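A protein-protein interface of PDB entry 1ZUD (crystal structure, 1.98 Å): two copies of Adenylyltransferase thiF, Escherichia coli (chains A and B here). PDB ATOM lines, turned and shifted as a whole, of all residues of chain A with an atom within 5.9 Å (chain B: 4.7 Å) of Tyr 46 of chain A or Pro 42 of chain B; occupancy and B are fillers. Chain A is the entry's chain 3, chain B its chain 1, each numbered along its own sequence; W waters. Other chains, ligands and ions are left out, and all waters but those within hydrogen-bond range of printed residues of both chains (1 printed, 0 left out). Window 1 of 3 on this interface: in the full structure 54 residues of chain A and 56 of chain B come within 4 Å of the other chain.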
ATOM      1  N   THR A  41     -25.538 -14.655   3.885  1.00  0.00           N
ATOM      2  CA  THR A  41     -24.382 -14.154   4.636  1.00  0.00           C
ATOM      3  C   THR A  41     -24.752 -13.733   6.083  1.00  0.00           C
ATOM      4  O   THR A  41     -24.047 -14.122   6.998  1.00  0.00           O
ATOM      5  CB  THR A  41     -23.664 -13.008   3.883  1.00  0.00           C
ATOM      6  OG1 THR A  41     -24.586 -11.970   3.578  1.00  0.00           O
ATOM      7  CG2 THR A  41     -23.062 -13.528   2.595  1.00  0.00           C
ATOM      8  N   PRO A  42     -25.849 -12.969   6.324  1.00  0.00           N
ATOM      9  CA  PRO A  42     -26.091 -12.673   7.758  1.00  0.00           C
ATOM     10  C   PRO A  42     -26.507 -13.929   8.511  1.00  0.00           C
ATOM     11  O   PRO A  42     -26.147 -14.090   9.689  1.00  0.00           O
ATOM     12  CB  PRO A  42     -27.216 -11.655   7.771  1.00  0.00           C
ATOM     13  CG  PRO A  42     -27.825 -11.781   6.416  1.00  0.00           C
ATOM     14  CD  PRO A  42     -26.814 -12.270   5.456  1.00  0.00           C
ATOM     15  N   ALA A  43     -27.274 -14.819   7.874  1.00  0.00           N
ATOM     16  CA  ALA A  43     -27.652 -16.033   8.606  1.00  0.00           C
ATOM     17  C   ALA A  43     -26.403 -16.813   9.041  1.00  0.00           C
ATOM     18  O   ALA A  43     -26.291 -17.278  10.187  1.00  0.00           O
ATOM     19  CB  ALA A  43     -28.567 -16.940   7.746  1.00  0.00           C
ATOM     20  N   ALA A  44     -25.440 -16.943   8.154  1.00  0.00           N
ATOM     21  CA  ALA A  44     -24.243 -17.697   8.526  1.00  0.00           C
ATOM     22  C   ALA A  44     -23.448 -16.979   9.666  1.00  0.00           C
ATOM     23  O   ALA A  44     -22.963 -17.641  10.591  1.00  0.00           O
ATOM     24  CB  ALA A  44     -23.330 -17.896   7.286  1.00  0.00           C
ATOM     25  N   LEU A  45     -23.333 -15.651   9.586  1.00  0.00           N
ATOM     26  CA  LEU A  45     -22.594 -14.876  10.592  1.00  0.00           C
ATOM     27  C   LEU A  45     -23.231 -15.113  11.959  1.00  0.00           C
ATOM     28  O   LEU A  45     -22.542 -15.372  12.925  1.00  0.00           O
ATOM     29  CB  LEU A  45     -22.636 -13.360  10.277  1.00  0.00           C
ATOM     30  CG  LEU A  45     -21.479 -12.905   9.368  1.00  0.00           C
ATOM     31  CD1 LEU A  45     -21.856 -11.607   8.635  1.00  0.00           C
ATOM     32  CD2 LEU A  45     -20.173 -12.799  10.200  1.00  0.00           C
ATOM     33  N   TYR A  46     -24.551 -14.982  12.043  1.00  0.00           N
ATOM     34  CA  TYR A  46     -25.231 -15.157  13.344  1.00  0.00           C
ATOM     35  C   TYR A  46     -25.207 -16.576  13.851  1.00  0.00           C
ATOM     36  O   TYR A  46     -25.134 -16.819  15.078  1.00  0.00           O
ATOM     37  CB  TYR A  46     -26.690 -14.651  13.282  1.00  0.00           C
ATOM     38  CG  TYR A  46     -26.745 -13.145  13.337  1.00  0.00           C
ATOM     39  CD1 TYR A  46     -26.977 -12.398  12.168  1.00  0.00           C
ATOM     40  CD2 TYR A  46     -26.438 -12.470  14.521  1.00  0.00           C
ATOM     41  CE1 TYR A  46     -26.876 -11.014  12.168  1.00  0.00           C
ATOM     42  CE2 TYR A  46     -26.366 -11.055  14.554  1.00  0.00           C
ATOM     43  CZ  TYR A  46     -26.585 -10.342  13.356  1.00  0.00           C
ATOM     44  OH  TYR A  46     -26.553  -8.972  13.360  1.00  0.00           O
ATOM     45  N   LEU A  47     -25.335 -17.524  12.937  1.00  0.00           N
ATOM     46  CA  LEU A  47     -25.312 -18.953  13.327  1.00  0.00           C
ATOM     47  C   LEU A  47     -23.885 -19.284  13.813  1.00  0.00           C
ATOM     48  O   LEU A  47     -23.699 -20.009  14.805  1.00  0.00           O
ATOM     49  CB  LEU A  47     -25.750 -19.803  12.136  1.00  0.00           C
ATOM     50  CG  LEU A  47     -27.194 -20.391  12.178  1.00  0.00           C
ATOM     51  CD1 LEU A  47     -28.053 -19.911  13.359  1.00  0.00           C
ATOM     52  CD2 LEU A  47     -27.842 -20.128  10.849  1.00  0.00           C
ATOM     53  N   ALA A  48     -22.874 -18.763  13.121  1.00  0.00           N
ATOM     54  CA  ALA A  48     -21.493 -18.988  13.600  1.00  0.00           C
ATOM     55  C   ALA A  48     -21.301 -18.350  14.990  1.00  0.00           C
ATOM     56  O   ALA A  48     -20.698 -18.954  15.905  1.00  0.00           O
ATOM     57  CB  ALA A  48     -20.485 -18.379  12.635  1.00  0.00           C
ATOM     58  N   GLY A  49     -21.793 -17.123  15.148  1.00  0.00           N
ATOM     59  CA  GLY A  49     -21.621 -16.458  16.422  1.00  0.00           C
ATOM     60  C   GLY A  49     -22.355 -17.194  17.510  1.00  0.00           C
ATOM     61  O   GLY A  49     -21.893 -17.192  18.657  1.00  0.00           O
ATOM     62  N   ALA A  50     -23.486 -17.817  17.168  1.00  0.00           N
ATOM     63  CA  ALA A  50     -24.308 -18.564  18.128  1.00  0.00           C
ATOM     64  C   ALA A  50     -23.730 -19.915  18.605  1.00  0.00           C
ATOM     65  O   ALA A  50     -24.254 -20.535  19.560  1.00  0.00           O
ATOM     66  CB  ALA A  50     -25.730 -18.841  17.506  1.00  0.00           C
ATOM     67  N   GLY A  51     -22.719 -20.416  17.907  1.00  0.00           N
ATOM     68  CA  GLY A  51     -22.155 -21.689  18.280  1.00  0.00           C
ATOM     69  C   GLY A  51     -22.802 -22.928  17.660  1.00  0.00           C
ATOM     70  O   GLY A  51     -22.753 -24.012  18.256  1.00  0.00           O
ATOM     71  N   ILE A  72     -22.808  -8.765   3.462  1.00  0.00           N
ATOM     72  CA  ILE A  72     -21.965  -8.235   4.544  1.00  0.00           C
ATOM     73  C   ILE A  72     -20.807  -9.032   5.080  1.00  0.00           C
ATOM     74  O   ILE A  72     -20.036  -8.530   5.908  1.00  0.00           O
ATOM     75  CB  ILE A  72     -22.831  -7.831   5.765  1.00  0.00           C
ATOM     76  CG1 ILE A  72     -23.429  -9.089   6.410  1.00  0.00           C
ATOM     77  CG2 ILE A  72     -23.917  -6.846   5.335  1.00  0.00           C
ATOM     78  CD1 ILE A  72     -24.370  -8.799   7.550  1.00  0.00           C
ATOM     79  N   LEU A  94     -14.216 -15.278  12.792  1.00  0.00           N
ATOM     80  CA  LEU A  94     -15.178 -14.907  13.817  1.00  0.00           C
ATOM     81  C   LEU A  94     -15.192 -15.978  14.917  1.00  0.00           C
ATOM     82  O   LEU A  94     -15.146 -15.696  16.125  1.00  0.00           O
ATOM     83  CB  LEU A  94     -16.570 -14.798  13.170  1.00  0.00           C
ATOM     84  CG  LEU A  94     -17.723 -14.556  14.145  1.00  0.00           C
ATOM     85  CD1 LEU A  94     -17.614 -13.162  14.802  1.00  0.00           C
ATOM     86  CD2 LEU A  94     -19.035 -14.715  13.369  1.00  0.00           C
ATOM     87  N   THR A 199     -31.397 -12.738   8.754  1.00  0.00           N
ATOM     88  CA  THR A 199     -31.136 -12.753  10.203  1.00  0.00           C
ATOM     89  C   THR A 199     -32.305 -13.484  10.902  1.00  0.00           C
ATOM     90  O   THR A 199     -32.100 -14.240  11.886  1.00  0.00           O
ATOM     91  CB  THR A 199     -31.002 -11.299  10.751  1.00  0.00           C
ATOM     92  OG1 THR A 199     -29.933 -10.678  10.044  1.00  0.00           O
ATOM     93  CG2 THR A 199     -30.643 -11.280  12.268  1.00  0.00           C
ATOM     94  N   ALA A 202     -31.818 -17.131  10.777  1.00  0.00           N
ATOM     95  CA  ALA A 202     -30.916 -17.610  11.854  1.00  0.00           C
ATOM     96  C   ALA A 202     -31.670 -17.765  13.196  1.00  0.00           C
ATOM     97  O   ALA A 202     -31.470 -18.729  13.951  1.00  0.00           O
ATOM     98  CB  ALA A 202     -29.679 -16.562  12.041  1.00  0.00           C
ATOM     99  N   ILE A 206     -32.003 -21.165  15.546  1.00  0.00           N
ATOM    100  CA  ILE A 206     -31.552 -21.282  16.916  1.00  0.00           C
ATOM    101  C   ILE A 206     -32.669 -21.781  17.795  1.00  0.00           C
ATOM    102  O   ILE A 206     -32.433 -22.607  18.669  1.00  0.00           O
ATOM    103  CB  ILE A 206     -31.047 -19.909  17.427  1.00  0.00           C
ATOM    104  CG1 ILE A 206     -29.776 -19.560  16.623  1.00  0.00           C
ATOM    105  CG2 ILE A 206     -30.735 -19.952  18.918  1.00  0.00           C
ATOM    106  CD1 ILE A 206     -29.385 -18.096  16.685  1.00  0.00           C
ATOM    107  N   GLY B  37     -22.131  -2.101  19.173  1.00  0.00           N
ATOM    108  CA  GLY B  37     -22.344  -3.438  19.743  1.00  0.00           C
ATOM    109  C   GLY B  37     -23.355  -4.220  18.904  1.00  0.00           C
ATOM    110  O   GLY B  37     -23.371  -4.119  17.672  1.00  0.00           O
ATOM    111  N   GLY B  38     -24.225  -4.972  19.572  1.00  0.00           N
ATOM    112  CA  GLY B  38     -25.209  -5.749  18.860  1.00  0.00           C
ATOM    113  C   GLY B  38     -26.041  -4.984  17.837  1.00  0.00           C
ATOM    114  O   GLY B  38     -26.370  -5.517  16.756  1.00  0.00           O
ATOM    115  N   LEU B  39     -26.426  -3.762  18.187  1.00  0.00           N
ATOM    116  CA  LEU B  39     -27.214  -2.936  17.286  1.00  0.00           C
ATOM    117  C   LEU B  39     -26.405  -2.205  16.268  1.00  0.00           C
ATOM    118  O   LEU B  39     -26.716  -2.200  15.086  1.00  0.00           O
ATOM    119  CB  LEU B  39     -27.994  -1.890  18.055  1.00  0.00           C
ATOM    120  CG  LEU B  39     -28.998  -2.377  19.088  1.00  0.00           C
ATOM    121  CD1 LEU B  39     -29.355  -1.177  19.941  1.00  0.00           C
ATOM    122  CD2 LEU B  39     -30.246  -2.991  18.409  1.00  0.00           C
ATOM    123  N   GLY B  40     -25.338  -1.580  16.734  1.00  0.00           N
ATOM    124  CA  GLY B  40     -24.535  -0.777  15.826  1.00  0.00           C
ATOM    125  C   GLY B  40     -23.728  -1.444  14.773  1.00  0.00           C
ATOM    126  O   GLY B  40     -23.530  -0.878  13.712  1.00  0.00           O
ATOM    127  N   THR B  41     -23.269  -2.671  15.023  1.00  0.00           N
ATOM    128  CA  THR B  41     -22.444  -3.276  14.020  1.00  0.00           C
ATOM    129  C   THR B  41     -23.244  -3.682  12.789  1.00  0.00           C
ATOM    130  O   THR B  41     -22.801  -3.420  11.673  1.00  0.00           O
ATOM    131  CB  THR B  41     -21.597  -4.462  14.601  1.00  0.00           C
ATOM    132  OG1 THR B  41     -22.440  -5.397  15.270  1.00  0.00           O
ATOM    133  CG2 THR B  41     -20.549  -3.916  15.597  1.00  0.00           C
ATOM    134  N   PRO B  42     -24.409  -4.356  12.954  1.00  0.00           N
ATOM    135  CA  PRO B  42     -25.080  -4.654  11.668  1.00  0.00           C
ATOM    136  C   PRO B  42     -25.500  -3.339  11.042  1.00  0.00           C
ATOM    137  O   PRO B  42     -25.378  -3.147   9.852  1.00  0.00           O
ATOM    138  CB  PRO B  42     -26.309  -5.549  12.076  1.00  0.00           C
ATOM    139  CG  PRO B  42     -26.529  -5.219  13.553  1.00  0.00           C
ATOM    140  CD  PRO B  42     -25.050  -5.077  14.072  1.00  0.00           C
ATOM    141  N   ALA B  43     -25.945  -2.372  11.835  1.00  0.00           N
ATOM    142  CA  ALA B  43     -26.374  -1.133  11.187  1.00  0.00           C
ATOM    143  C   ALA B  43     -25.277  -0.449  10.383  1.00  0.00           C
ATOM    144  O   ALA B  43     -25.510   0.060   9.257  1.00  0.00           O
ATOM    145  CB  ALA B  43     -26.975  -0.124  12.243  1.00  0.00           C
ATOM    146  N   ALA B  44     -24.079  -0.421  10.947  1.00  0.00           N
ATOM    147  CA  ALA B  44     -22.976   0.236  10.235  1.00  0.00           C
ATOM    148  C   ALA B  44     -22.611  -0.546   8.992  1.00  0.00           C
ATOM    149  O   ALA B  44     -22.292   0.037   7.972  1.00  0.00           O
ATOM    150  CB  ALA B  44     -21.737   0.351  11.149  1.00  0.00           C
ATOM    151  N   LEU B  45     -22.628  -1.865   9.078  1.00  0.00           N
ATOM    152  CA  LEU B  45     -22.305  -2.661   7.904  1.00  0.00           C
ATOM    153  C   LEU B  45     -23.273  -2.380   6.746  1.00  0.00           C
ATOM    154  O   LEU B  45     -22.816  -2.283   5.614  1.00  0.00           O
ATOM    155  CB  LEU B  45     -22.346  -4.160   8.217  1.00  0.00           C
ATOM    156  CG  LEU B  45     -21.074  -4.815   8.775  1.00  0.00           C
ATOM    157  CD1 LEU B  45     -21.422  -6.118   9.555  1.00  0.00           C
ATOM    158  CD2 LEU B  45     -20.098  -5.102   7.588  1.00  0.00           C
ATOM    159  N   TYR B  46     -24.592  -2.278   7.017  1.00  0.00           N
ATOM    160  CA  TYR B  46     -25.545  -2.058   5.963  1.00  0.00           C
ATOM    161  C   TYR B  46     -25.481  -0.661   5.463  1.00  0.00           C
ATOM    162  O   TYR B  46     -25.630  -0.420   4.290  1.00  0.00           O
ATOM    163  CB  TYR B  46     -26.980  -2.408   6.451  1.00  0.00           C
ATOM    164  CG  TYR B  46     -27.187  -3.921   6.445  1.00  0.00           C
ATOM    165  CD1 TYR B  46     -27.142  -4.639   7.602  1.00  0.00           C
ATOM    166  CD2 TYR B  46     -27.365  -4.608   5.240  1.00  0.00           C
ATOM    167  CE1 TYR B  46     -27.293  -6.056   7.604  1.00  0.00           C
ATOM    168  CE2 TYR B  46     -27.505  -6.004   5.205  1.00  0.00           C
ATOM    169  CZ  TYR B  46     -27.477  -6.726   6.398  1.00  0.00           C
ATOM    170  OH  TYR B  46     -27.625  -8.116   6.376  1.00  0.00           O
ATOM    171  N   ARG B  70     -22.680 -11.704  18.980  1.00  0.00           N
ATOM    172  CA  ARG B  70     -23.655 -10.818  18.351  1.00  0.00           C
ATOM    173  C   ARG B  70     -23.108  -9.579  17.659  1.00  0.00           C
ATOM    174  O   ARG B  70     -23.838  -8.882  16.933  1.00  0.00           O
ATOM    175  CB  ARG B  70     -24.702 -10.405  19.402  1.00  0.00           C
ATOM    176  CG  ARG B  70     -24.120  -9.597  20.516  1.00  0.00           C
ATOM    177  CD  ARG B  70     -25.020  -9.569  21.692  1.00  0.00           C
ATOM    178  NE  ARG B  70     -24.413  -8.746  22.734  1.00  0.00           N
ATOM    179  CZ  ARG B  70     -23.332  -9.104  23.417  1.00  0.00           C
ATOM    180  NH1 ARG B  70     -22.730 -10.275  23.174  1.00  0.00           N
ATOM    181  NH2 ARG B  70     -22.864  -8.290  24.348  1.00  0.00           N
ATOM    182  N   ILE B  72     -21.207  -8.809  14.966  1.00  0.00           N
ATOM    183  CA  ILE B  72     -20.748  -9.439  13.722  1.00  0.00           C
ATOM    184  C   ILE B  72     -19.699  -8.766  12.865  1.00  0.00           C
ATOM    185  O   ILE B  72     -19.206  -9.359  11.904  1.00  0.00           O
ATOM    186  CB  ILE B  72     -21.974  -9.773  12.787  1.00  0.00           C
ATOM    187  CG1 ILE B  72     -22.695  -8.480  12.384  1.00  0.00           C
ATOM    188  CG2 ILE B  72     -22.875 -10.717  13.497  1.00  0.00           C
ATOM    189  CD1 ILE B  72     -23.545  -8.616  11.172  1.00  0.00           C
ATOM    190  N   GLY B 191     -28.376 -13.352  19.610  1.00  0.00           N
ATOM    191  CA  GLY B 191     -27.748 -12.541  18.580  1.00  0.00           C
ATOM    192  C   GLY B 191     -28.633 -12.051  17.461  1.00  0.00           C
ATOM    193  O   GLY B 191     -28.682 -10.848  17.194  1.00  0.00           O
ATOM    194  N   PRO B 192     -29.399 -12.962  16.811  1.00  0.00           N
ATOM    195  CA  PRO B 192     -30.228 -12.437  15.731  1.00  0.00           C
ATOM    196  C   PRO B 192     -31.367 -11.526  16.173  1.00  0.00           C
ATOM    197  O   PRO B 192     -31.916 -10.777  15.347  1.00  0.00           O
ATOM    198  CB  PRO B 192     -30.675 -13.706  14.932  1.00  0.00           C
ATOM    199  CG  PRO B 192     -30.280 -14.890  15.766  1.00  0.00           C
ATOM    200  CD  PRO B 192     -29.198 -14.422  16.752  1.00  0.00           C
ATOM    201  N   GLY B 195     -29.632  -8.232  16.346  1.00  0.00           N
ATOM    202  CA  GLY B 195     -29.238  -8.026  14.959  1.00  0.00           C
ATOM    203  C   GLY B 195     -30.396  -7.559  14.067  1.00  0.00           C
ATOM    204  O   GLY B 195     -30.225  -6.632  13.274  1.00  0.00           O
ATOM    205  N   GLY B 198     -30.951  -3.816  14.861  1.00  0.00           N
ATOM    206  CA  GLY B 198     -29.943  -2.900  14.327  1.00  0.00           C
ATOM    207  C   GLY B 198     -30.075  -2.779  12.796  1.00  0.00           C
ATOM    208  O   GLY B 198     -29.905  -1.699  12.198  1.00  0.00           O
ATOM    209  N   THR B 199     -30.408  -3.891  12.148  1.00  0.00           N
ATOM    210  CA  THR B 199     -30.562  -3.885  10.690  1.00  0.00           C
ATOM    211  C   THR B 199     -31.766  -3.044  10.313  1.00  0.00           C
ATOM    212  O   THR B 199     -31.736  -2.313   9.313  1.00  0.00           O
ATOM    213  CB  THR B 199     -30.709  -5.324  10.134  1.00  0.00           C
ATOM    214  OG1 THR B 199     -29.561  -6.084  10.530  1.00  0.00           O
ATOM    215  CG2 THR B 199     -30.791  -5.317   8.611  1.00  0.00           C
HETATM  216  O   HOH W   1     -26.037  -8.022  15.965  1.00  0.00           O
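OG1 of Thr 199 of chain B lies within hydrogen-bond range of O of Gly 195 of chain B (2.9 Å).
Pro 42 of chain A touches Tyr 46 of chain B (CG to OH, 3.7 Å). Leu 45 of chain A touches Ile 72 of chain B. Pro 42 of chain B touches Tyr 46 of chain A. CG2 of Ile 72 of chain B touches CE2 of Tyr 46 of chain A, at 3.7 Å. Tyr 46 of chain A touches Pro 192 of chain B. OH of Tyr 46 of chain A touches CA of Gly 195 of chain B, at 3.3 Å. Ile 72 of chain A touches Tyr 46 of chain B (CD1 to OH, 3.5 Å). CD1 of Ile 72 of chain A touches CD1 of Ile 72 of chain B (3.7 Å). Thr 199 of chain A touches Pro 192 of chain B. Ile 206 of chain A touches Pro 192 of chain B.
Tyr 46 of chain A touches five residues of chain B. Pro 42 of chain B touches one residue of chain A. Printed residues of chain A within 4 Å of Pro 192 of chain B: Tyr 46, Thr 199 and Ile 206. Printed residues of chain A within 4 Å of Gly 195 of chain B: Tyr 46. Of the printed residues of chain A, Leu 45 of chain B touches Ile 72 (3.8 Å). Of the printed residues of chain B, Pro 42 of chain A touches Tyr 46. Of the printed residues of chain B, Ile 206 of chain A touches Pro 192. Leu 39 of chain B touches none of the printed residues of chain A. Ala 48 of chain A touches none of the printed residues of chain B. The nearest residue of chain B that does not touch Tyr 46 of chain A is Arg 70 of chain B (4.1 Å). The nearest printed residue of chain A that does not touch Pro 42 of chain B is Ile 72 of chain A (5.9 Å). The nearest printed residue of chain A that does not touch Tyr 46 of chain B is Thr 199 of chain A (5.0 Å).
Of the 17 printed residues of chain B, 7 touch a printed residue of chain A. Hydrophobic or aromatic side chains of chain B that line the printed part of chain A: Pro 42, Leu 45, Tyr 46, Ile 72 and Pro 192. Among the printed residues, 12 pairs touch across the chains.
Pro 42 of chain A touches Tyr 46 of chain B, and with the chains exchanged Tyr 46 of chain A touches Pro 42 of chain B. Leu 45 of chain A touches Ile 72 of chain B, and with the chains exchanged Ile 72 of chain A touches Leu 45 of chain B. Tyr 46 of chain A touches Ile 72 of chain B, and with the chains exchanged Ile 72 of chain A touches Tyr 46 of chain B. Ile 72 of chain B touches its own counterpart, Ile 72 of chain A. Positions printed for both chains: 41, 42, 43, 44, 45, 46, 72 and 199. Of the 12 pairs that touch across the chains among the printed residues, 7 have their exchanged pair printed and touching as well.
Water W1 lies within hydrogen-bond range of O of Arg 70 of chain B, O of Gly 38 of chain B and OH of Tyr 46 of chain A.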
